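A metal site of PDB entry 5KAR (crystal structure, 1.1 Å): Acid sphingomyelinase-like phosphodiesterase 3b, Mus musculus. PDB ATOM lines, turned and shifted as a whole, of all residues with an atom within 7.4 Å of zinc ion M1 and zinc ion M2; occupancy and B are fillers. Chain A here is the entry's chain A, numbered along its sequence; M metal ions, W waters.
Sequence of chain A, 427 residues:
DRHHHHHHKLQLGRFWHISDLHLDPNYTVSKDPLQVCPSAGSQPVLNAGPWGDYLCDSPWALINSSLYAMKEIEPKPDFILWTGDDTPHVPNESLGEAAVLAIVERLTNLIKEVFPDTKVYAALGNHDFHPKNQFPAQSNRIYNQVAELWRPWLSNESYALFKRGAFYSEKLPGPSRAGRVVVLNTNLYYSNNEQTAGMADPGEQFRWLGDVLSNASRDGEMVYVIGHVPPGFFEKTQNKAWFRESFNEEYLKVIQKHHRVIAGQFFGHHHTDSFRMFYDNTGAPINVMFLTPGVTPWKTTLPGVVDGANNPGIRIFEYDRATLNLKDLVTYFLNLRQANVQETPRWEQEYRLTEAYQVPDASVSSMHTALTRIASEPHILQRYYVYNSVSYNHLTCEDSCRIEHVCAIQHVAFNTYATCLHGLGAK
Within 4 Å of zinc ion M1: Asp 20, Asp 85, Asn 126, His 228 and His 269.
Within 4 Å of zinc ion M2: Asp 20, His 22, Asp 85, His 269 and His 271.
Zinc ion M2 is bound by water W1 (2.0 Å), the side-chain carboxylate of Asp 20 (2.0 Å), a ring nitrogen (NE2) of His 22 (2.1 Å), a ring nitrogen (NE2) of His 271 (2.1 Å) and the side-chain carboxylate of Asp 85 (2.3 Å).
Zinc ion M1 is bound by water W1 (2.0 Å), OD1 of Asn 126 (2.1 Å), NE2 of His 228 (2.1 Å), ND1 of His 269 (2.1 Å) and OD2 of Asp 85 (2.2 Å).
The backbone NH (N) of His 269 sits at hydrogen-bond distance from the side-chain carboxylate (OD2) of Asp 20, at 3.0 Å. N of Thr 296 lies within hydrogen-bond range of O of Asp 20 (3.1 Å). N of Asp 20 lies within hydrogen-bond range of O of Gly 84, at 2.8 Å. The side-chain carboxylate (OD2) of Asp 20 is in hydrogen-bond range of the side-chain hydroxyl (OG) of Ser 19 (2.7 Å). The side-chain amide nitrogen of Asn 126 lies within hydrogen-bond range of the side-chain amide oxygen of Asn 133, 2.8 Å away. The backbone NH (N) of Gly 294 lies within hydrogen-bond range of the backbone carbonyl oxygen (O) of His 271 (3.0 Å). A ring nitrogen (ND1) of His 228 sits at hydrogen-bond distance from the backbone carbonyl oxygen (O) of Thr 83. The side-chain carboxylate (OD1) of Asp 85 sits at hydrogen-bond distance from the backbone NH (N) of His 127, at 2.9 Å.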
ATOM      1  N   SER A  19      -8.350   8.786 -22.837  1.00  0.00           N
ATOM      2  CA  SER A  19      -8.545  10.178 -22.471  1.00  0.00           C
ATOM      3  C   SER A  19      -7.489  11.051 -23.133  1.00  0.00           C
ATOM      4  O   SER A  19      -6.384  10.604 -23.451  1.00  0.00           O
ATOM      5  CB  SER A  19      -8.436  10.337 -20.961  1.00  0.00           C
ATOM      6  OG  SER A  19      -9.076  11.507 -20.499  1.00  0.00           O
ATOM      7  N   ASP A  20      -7.840  12.327 -23.303  1.00  0.00           N
ATOM      8  CA  ASP A  20      -6.885  13.355 -23.655  1.00  0.00           C
ATOM      9  C   ASP A  20      -6.161  13.022 -24.958  1.00  0.00           C
ATOM     10  O   ASP A  20      -4.951  13.043 -25.040  1.00  0.00           O
ATOM     11  CB  ASP A  20      -5.933  13.633 -22.507  1.00  0.00           C
ATOM     12  CG  ASP A  20      -6.686  14.188 -21.298  1.00  0.00           C
ATOM     13  OD1 ASP A  20      -6.800  15.422 -21.181  1.00  0.00           O
ATOM     14  OD2 ASP A  20      -7.132  13.405 -20.438  1.00  0.00           O
ATOM     15  N   LEU A  21      -6.949  12.750 -25.996  1.00  0.00           N
ATOM     16  CA  LEU A  21      -6.429  12.481 -27.322  1.00  0.00           C
ATOM     17  C   LEU A  21      -5.863  13.738 -27.965  1.00  0.00           C
ATOM     18  O   LEU A  21      -4.917  13.637 -28.743  1.00  0.00           O
ATOM     19  CB  LEU A  21      -7.495  11.806 -28.176  1.00  0.00           C
ATOM     20  CG  LEU A  21      -7.601  10.287 -27.988  1.00  0.00           C
ATOM     21  CD1 LEU A  21      -7.776   9.814 -26.553  1.00  0.00           C
ATOM     22  CD2 LEU A  21      -8.695   9.725 -28.909  1.00  0.00           C
ATOM     23  N   HIS A  22      -6.458  14.905 -27.717  1.00  0.00           N
ATOM     24  CA  HIS A  22      -5.993  16.213 -28.177  1.00  0.00           C
ATOM     25  C   HIS A  22      -5.419  16.182 -29.601  1.00  0.00           C
ATOM     26  O   HIS A  22      -4.212  16.326 -29.809  1.00  0.00           O
ATOM     27  CB  HIS A  22      -4.925  16.787 -27.233  1.00  0.00           C
ATOM     28  CG  HIS A  22      -5.414  17.203 -25.882  1.00  0.00           C
ATOM     29  ND1 HIS A  22      -6.147  18.352 -25.664  1.00  0.00           N
ATOM     30  CD2 HIS A  22      -5.210  16.665 -24.663  1.00  0.00           C
ATOM     31  CE1 HIS A  22      -6.384  18.489 -24.368  1.00  0.00           C
ATOM     32  NE2 HIS A  22      -5.847  17.473 -23.730  1.00  0.00           N
ATOM     33  N   ASP A  57       0.675  18.344 -29.680  1.00  0.00           N
ATOM     34  CA  ASP A  57      -0.477  17.476 -29.544  1.00  0.00           C
ATOM     35  C   ASP A  57      -0.527  16.452 -30.698  1.00  0.00           C
ATOM     36  O   ASP A  57       0.304  16.456 -31.610  1.00  0.00           O
ATOM     37  CB  ASP A  57      -1.753  18.319 -29.459  1.00  0.00           C
ATOM     38  CG  ASP A  57      -2.024  18.833 -28.067  1.00  0.00           C
ATOM     39  OD1 ASP A  57      -1.899  18.060 -27.080  1.00  0.00           O
ATOM     40  OD2 ASP A  57      -2.389  20.025 -27.969  1.00  0.00           O
ATOM     41  N   THR A  83     -12.930   9.936 -21.575  1.00  0.00           N
ATOM     42  CA  THR A  83     -13.097  11.103 -20.715  1.00  0.00           C
ATOM     43  C   THR A  83     -12.592  12.409 -21.328  1.00  0.00           C
ATOM     44  O   THR A  83     -12.240  13.324 -20.589  1.00  0.00           O
ATOM     45  CB  THR A  83     -12.552  10.815 -19.313  1.00  0.00           C
ATOM     46  OG1 THR A  83     -11.224  10.292 -19.373  1.00  0.00           O
ATOM     47  CG2 THR A  83     -13.378   9.790 -18.605  1.00  0.00           C
ATOM     48  N   GLY A  84     -12.560  12.531 -22.665  1.00  0.00           N
ATOM     49  CA  GLY A  84     -12.568  13.823 -23.311  1.00  0.00           C
ATOM     50  C   GLY A  84     -11.214  14.461 -23.502  1.00  0.00           C
ATOM     51  O   GLY A  84     -10.158  13.879 -23.258  1.00  0.00           O
ATOM     52  N   ASP A  85     -11.282  15.718 -23.943  1.00  0.00           N
ATOM     53  CA  ASP A  85     -10.155  16.593 -24.324  1.00  0.00           C
ATOM     54  C   ASP A  85      -9.625  16.204 -25.698  1.00  0.00           C
ATOM     55  O   ASP A  85      -8.602  15.518 -25.839  1.00  0.00           O
ATOM     56  CB  ASP A  85      -9.049  16.634 -23.276  1.00  0.00           C
ATOM     57  CG  ASP A  85      -9.064  17.881 -22.413  1.00  0.00           C
ATOM     58  OD1 ASP A  85     -10.035  18.643 -22.468  1.00  0.00           O
ATOM     59  OD2 ASP A  85      -8.052  18.073 -21.683  1.00  0.00           O
ATOM     60  N   ASP A  86     -10.298  16.701 -26.728  1.00  0.00           N
ATOM     61  CA  ASP A  86     -10.126  16.251 -28.090  1.00  0.00           C
ATOM     62  C   ASP A  86      -9.401  17.233 -28.985  1.00  0.00           C
ATOM     63  O   ASP A  86      -9.001  16.861 -30.114  1.00  0.00           O
ATOM     64  CB  ASP A  86     -11.492  15.990 -28.736  1.00  0.00           C
ATOM     65  CG  ASP A  86     -12.355  15.021 -27.946  1.00  0.00           C
ATOM     66  OD1 ASP A  86     -11.835  14.248 -27.129  1.00  0.00           O
ATOM     67  OD2 ASP A  86     -13.587  15.032 -28.216  1.00  0.00           O
ATOM     68  N   THR A  87      -9.283  18.486 -28.567  1.00  0.00           N
ATOM     69  CA  THR A  87      -8.821  19.586 -29.384  1.00  0.00           C
ATOM     70  C   THR A  87      -7.450  20.025 -28.901  1.00  0.00           C
ATOM     71  O   THR A  87      -6.998  19.659 -27.818  1.00  0.00           O
ATOM     72  CB  THR A  87      -9.810  20.748 -29.234  1.00  0.00           C
ATOM     73  OG1 THR A  87      -9.796  21.113 -27.865  1.00  0.00           O
ATOM     74  CG2 THR A  87     -11.224  20.357 -29.636  1.00  0.00           C
ATOM     75  N   HIS A  89      -4.002  22.392 -27.832  1.00  0.00           N
ATOM     76  CA  HIS A  89      -3.640  23.469 -26.921  1.00  0.00           C
ATOM     77  C   HIS A  89      -3.148  24.651 -27.749  1.00  0.00           C
ATOM     78  O   HIS A  89      -1.948  24.812 -28.005  1.00  0.00           O
ATOM     79  CB  HIS A  89      -2.559  23.010 -25.959  1.00  0.00           C
ATOM     80  CG  HIS A  89      -2.976  21.905 -25.050  1.00  0.00           C
ATOM     81  ND1 HIS A  89      -2.937  20.592 -25.434  1.00  0.00           N
ATOM     82  CD2 HIS A  89      -3.463  21.913 -23.782  1.00  0.00           C
ATOM     83  CE1 HIS A  89      -3.345  19.822 -24.437  1.00  0.00           C
ATOM     84  NE2 HIS A  89      -3.680  20.596 -23.438  1.00  0.00           N
ATOM     85  N   GLY A 125     -14.261  17.007 -22.022  1.00  0.00           N
ATOM     86  CA  GLY A 125     -13.139  17.600 -21.349  1.00  0.00           C
ATOM     87  C   GLY A 125     -13.120  19.110 -21.502  1.00  0.00           C
ATOM     88  O   GLY A 125     -13.860  19.681 -22.291  1.00  0.00           O
ATOM     89  N   ASN A 126     -12.213  19.750 -20.754  1.00  0.00           N
ATOM     90  CA  ASN A 126     -12.249  21.206 -20.645  1.00  0.00           C
ATOM     91  C   ASN A 126     -11.905  21.903 -21.959  1.00  0.00           C
ATOM     92  O   ASN A 126     -12.333  23.055 -22.161  1.00  0.00           O
ATOM     93  CB  ASN A 126     -11.375  21.687 -19.483  1.00  0.00           C
ATOM     94  CG  ASN A 126      -9.922  21.272 -19.626  1.00  0.00           C
ATOM     95  OD1 ASN A 126      -9.614  20.103 -19.608  1.00  0.00           O
ATOM     96  ND2 ASN A 126      -9.016  22.244 -19.768  1.00  0.00           N
ATOM     97  N   HIS A 127     -11.173  21.240 -22.835  1.00  0.00           N
ATOM     98  CA  HIS A 127     -10.873  21.769 -24.159  1.00  0.00           C
ATOM     99  C   HIS A 127     -11.956  21.490 -25.180  1.00  0.00           C
ATOM    100  O   HIS A 127     -11.861  22.006 -26.320  1.00  0.00           O
ATOM    101  CB  HIS A 127      -9.552  21.188 -24.655  1.00  0.00           C
ATOM    102  CG  HIS A 127      -8.372  21.775 -23.971  1.00  0.00           C
ATOM    103  ND1 HIS A 127      -7.727  22.901 -24.425  1.00  0.00           N
ATOM    104  CD2 HIS A 127      -7.765  21.442 -22.813  1.00  0.00           C
ATOM    105  CE1 HIS A 127      -6.759  23.224 -23.594  1.00  0.00           C
ATOM    106  NE2 HIS A 127      -6.764  22.364 -22.592  1.00  0.00           N
ATOM    107  N   ASN A 133     -12.644  25.878 -21.612  1.00  0.00           N
ATOM    108  CA  ASN A 133     -12.895  25.865 -20.186  1.00  0.00           C
ATOM    109  C   ASN A 133     -14.202  26.538 -19.793  1.00  0.00           C
ATOM    110  O   ASN A 133     -14.580  26.426 -18.652  1.00  0.00           O
ATOM    111  CB  ASN A 133     -11.755  26.491 -19.351  1.00  0.00           C
ATOM    112  CG  ASN A 133     -10.423  25.898 -19.684  1.00  0.00           C
ATOM    113  OD1 ASN A 133     -10.313  24.692 -19.897  1.00  0.00           O
ATOM    114  ND2 ASN A 133      -9.419  26.740 -19.790  1.00  0.00           N
ATOM    115  N   ASN A 187     -15.930  19.957 -15.671  1.00  0.00           N
ATOM    116  CA  ASN A 187     -15.473  21.246 -16.187  1.00  0.00           C
ATOM    117  C   ASN A 187     -16.244  22.392 -15.561  1.00  0.00           C
ATOM    118  O   ASN A 187     -15.744  23.527 -15.546  1.00  0.00           O
ATOM    119  CB  ASN A 187     -15.599  21.242 -17.713  1.00  0.00           C
ATOM    120  CG  ASN A 187     -15.026  19.982 -18.322  1.00  0.00           C
ATOM    121  OD1 ASN A 187     -13.833  19.711 -18.206  1.00  0.00           O
ATOM    122  ND2 ASN A 187     -15.877  19.182 -18.899  1.00  0.00           N
ATOM    123  N   TYR A 190     -13.901  23.845 -12.701  1.00  0.00           N
ATOM    124  CA  TYR A 190     -12.567  24.356 -12.932  1.00  0.00           C
ATOM    125  C   TYR A 190     -12.512  25.847 -12.575  1.00  0.00           C
ATOM    126  O   TYR A 190     -13.384  26.630 -12.940  1.00  0.00           O
ATOM    127  CB  TYR A 190     -12.208  24.091 -14.408  1.00  0.00           C
ATOM    128  CG  TYR A 190     -10.780  24.314 -14.857  1.00  0.00           C
ATOM    129  CD1 TYR A 190      -9.732  24.602 -13.969  1.00  0.00           C
ATOM    130  CD2 TYR A 190     -10.474  24.305 -16.203  1.00  0.00           C
ATOM    131  CE1 TYR A 190      -8.440  24.824 -14.423  1.00  0.00           C
ATOM    132  CE2 TYR A 190      -9.205  24.527 -16.647  1.00  0.00           C
ATOM    133  CZ  TYR A 190      -8.201  24.787 -15.768  1.00  0.00           C
ATOM    134  OH  TYR A 190      -6.922  25.015 -16.263  1.00  0.00           O
ATOM    135  N   HIS A 228     -13.740  14.299 -16.456  1.00  0.00           N
ATOM    136  CA  HIS A 228     -12.493  14.763 -17.040  1.00  0.00           C
ATOM    137  C   HIS A 228     -11.566  15.359 -15.984  1.00  0.00           C
ATOM    138  O   HIS A 228     -10.505  14.780 -15.718  1.00  0.00           O
ATOM    139  CB  HIS A 228     -12.724  15.761 -18.164  1.00  0.00           C
ATOM    140  CG  HIS A 228     -11.452  16.212 -18.771  1.00  0.00           C
ATOM    141  ND1 HIS A 228     -10.711  15.373 -19.574  1.00  0.00           N
ATOM    142  CD2 HIS A 228     -10.724  17.330 -18.597  1.00  0.00           C
ATOM    143  CE1 HIS A 228      -9.587  15.987 -19.913  1.00  0.00           C
ATOM    144  NE2 HIS A 228      -9.578  17.180 -19.349  1.00  0.00           N
ATOM    145  N   VAL A 229     -11.924  16.514 -15.422  1.00  0.00           N
ATOM    146  CA  VAL A 229     -11.089  17.222 -14.446  1.00  0.00           C
ATOM    147  C   VAL A 229     -11.267  16.546 -13.089  1.00  0.00           C
ATOM    148  O   VAL A 229     -12.412  16.460 -12.597  1.00  0.00           O
ATOM    149  CB  VAL A 229     -11.487  18.704 -14.354  1.00  0.00           C
ATOM    150  CG1 VAL A 229     -10.569  19.423 -13.362  1.00  0.00           C
ATOM    151  CG2 VAL A 229     -11.433  19.394 -15.712  1.00  0.00           C
ATOM    152  N   PRO A 230     -10.195  16.144 -12.422  1.00  0.00           N
ATOM    153  CA  PRO A 230     -10.335  15.511 -11.095  1.00  0.00           C
ATOM    154  C   PRO A 230     -10.302  16.536  -9.993  1.00  0.00           C
ATOM    155  O   PRO A 230      -9.753  17.636 -10.180  1.00  0.00           O
ATOM    156  CB  PRO A 230      -9.087  14.633 -11.014  1.00  0.00           C
ATOM    157  CG  PRO A 230      -8.073  15.409 -11.772  1.00  0.00           C
ATOM    158  CD  PRO A 230      -8.804  16.056 -12.924  1.00  0.00           C
ATOM    159  N   GLY A 268      -9.205  11.951 -16.118  1.00  0.00           N
ATOM    160  CA  GLY A 268      -8.087  12.242 -16.994  1.00  0.00           C
ATOM    161  C   GLY A 268      -7.476  13.606 -16.665  1.00  0.00           C
ATOM    162  O   GLY A 268      -7.209  13.876 -15.484  1.00  0.00           O
ATOM    163  N   HIS A 269      -7.310  14.455 -17.685  1.00  0.00           N
ATOM    164  CA  HIS A 269      -6.872  15.840 -17.594  1.00  0.00           C
ATOM    165  C   HIS A 269      -5.393  16.031 -17.329  1.00  0.00           C
ATOM    166  O   HIS A 269      -4.783  16.919 -17.932  1.00  0.00           O
ATOM    167  CB  HIS A 269      -7.738  16.601 -16.578  1.00  0.00           C
ATOM    168  CG  HIS A 269      -7.442  18.065 -16.495  1.00  0.00           C
ATOM    169  ND1 HIS A 269      -7.607  18.935 -17.553  1.00  0.00           N
ATOM    170  CD2 HIS A 269      -6.944  18.788 -15.466  1.00  0.00           C
ATOM    171  CE1 HIS A 269      -7.264  20.146 -17.156  1.00  0.00           C
ATOM    172  NE2 HIS A 269      -6.870  20.090 -15.891  1.00  0.00           N
ATOM    173  N   HIS A 270      -4.787  15.205 -16.501  1.00  0.00           N
ATOM    174  CA  HIS A 270      -3.382  15.382 -16.170  1.00  0.00           C
ATOM    175  C   HIS A 270      -2.457  14.920 -17.290  1.00  0.00           C
ATOM    176  O   HIS A 270      -1.357  15.440 -17.395  1.00  0.00           O
ATOM    177  CB  HIS A 270      -3.034  14.622 -14.926  1.00  0.00           C
ATOM    178  CG  HIS A 270      -3.625  15.231 -13.698  1.00  0.00           C
ATOM    179  ND1 HIS A 270      -3.618  14.584 -12.482  1.00  0.00           N
ATOM    180  CD2 HIS A 270      -4.221  16.421 -13.486  1.00  0.00           C
ATOM    181  CE1 HIS A 270      -4.183  15.359 -11.574  1.00  0.00           C
ATOM    182  NE2 HIS A 270      -4.576  16.469 -12.153  1.00  0.00           N
ATOM    183  N   HIS A 271      -2.850  13.910 -18.032  1.00  0.00           N
ATOM    184  CA  HIS A 271      -2.094  13.225 -19.086  1.00  0.00           C
ATOM    185  C   HIS A 271      -1.090  12.246 -18.525  1.00  0.00           C
ATOM    186  O   HIS A 271      -0.487  11.482 -19.285  1.00  0.00           O
ATOM    187  CB  HIS A 271      -1.396  14.153 -20.087  1.00  0.00           C
ATOM    188  CG  HIS A 271      -2.309  15.137 -20.726  1.00  0.00           C
ATOM    189  ND1 HIS A 271      -1.861  16.088 -21.609  1.00  0.00           N
ATOM    190  CD2 HIS A 271      -3.645  15.336 -20.608  1.00  0.00           C
ATOM    191  CE1 HIS A 271      -2.888  16.828 -22.011  1.00  0.00           C
ATOM    192  NE2 HIS A 271      -3.990  16.396 -21.413  1.00  0.00           N
ATOM    193  N   GLY A 294      -2.661  10.305 -21.006  1.00  0.00           N
ATOM    194  CA  GLY A 294      -3.217  10.730 -22.274  1.00  0.00           C
ATOM    195  C   GLY A 294      -2.582  10.054 -23.464  1.00  0.00           C
ATOM    196  O   GLY A 294      -1.466   9.538 -23.398  1.00  0.00           O
ATOM    197  N   THR A 296      -2.189  12.074 -26.135  1.00  0.00           N
ATOM    198  CA  THR A 296      -1.294  13.149 -26.551  1.00  0.00           C
ATOM    199  C   THR A 296      -0.003  13.092 -25.734  1.00  0.00           C
ATOM    200  O   THR A 296      -0.045  12.834 -24.522  1.00  0.00           O
ATOM    201  CB  THR A 296      -1.943  14.522 -26.412  1.00  0.00           C
ATOM    202  OG1 THR A 296      -1.110  15.451 -27.110  1.00  0.00           O
ATOM    203  CG2 THR A 296      -2.093  14.973 -24.967  1.00  0.00           C
ATOM    204  N   TRP A 298       2.068  15.777 -25.568  1.00  0.00           N
ATOM    205  CA  TRP A 298       2.369  17.214 -25.491  1.00  0.00           C
ATOM    206  C   TRP A 298       3.047  17.635 -24.186  1.00  0.00           C
ATOM    207  O   TRP A 298       2.513  17.445 -23.090  1.00  0.00           O
ATOM    208  CB  TRP A 298       1.030  17.935 -25.632  1.00  0.00           C
ATOM    209  CG  TRP A 298       1.012  19.417 -25.525  1.00  0.00           C
ATOM    210  CD1 TRP A 298       1.369  20.298 -26.469  1.00  0.00           C
ATOM    211  CD2 TRP A 298       0.543  20.173 -24.423  1.00  0.00           C
ATOM    212  NE1 TRP A 298       1.185  21.585 -26.024  1.00  0.00           N
ATOM    213  CE2 TRP A 298       0.671  21.538 -24.760  1.00  0.00           C
ATOM    214  CE3 TRP A 298       0.022  19.834 -23.176  1.00  0.00           C
ATOM    215  CZ2 TRP A 298       0.292  22.557 -23.901  1.00  0.00           C
ATOM    216  CZ3 TRP A 298      -0.357  20.855 -22.328  1.00  0.00           C
ATOM    217  CH2 TRP A 298      -0.209  22.200 -22.688  1.00  0.00           C
HETATM  218 ZN    ZN M   1      -8.124  18.668 -19.606  1.00  0.00          ZN
HETATM  219 ZN    ZN M   2      -5.909  17.167 -21.698  1.00  0.00          ZN
HETATM  220  O   HOH W   1      -6.181  18.223 -20.067  1.00  0.00           O
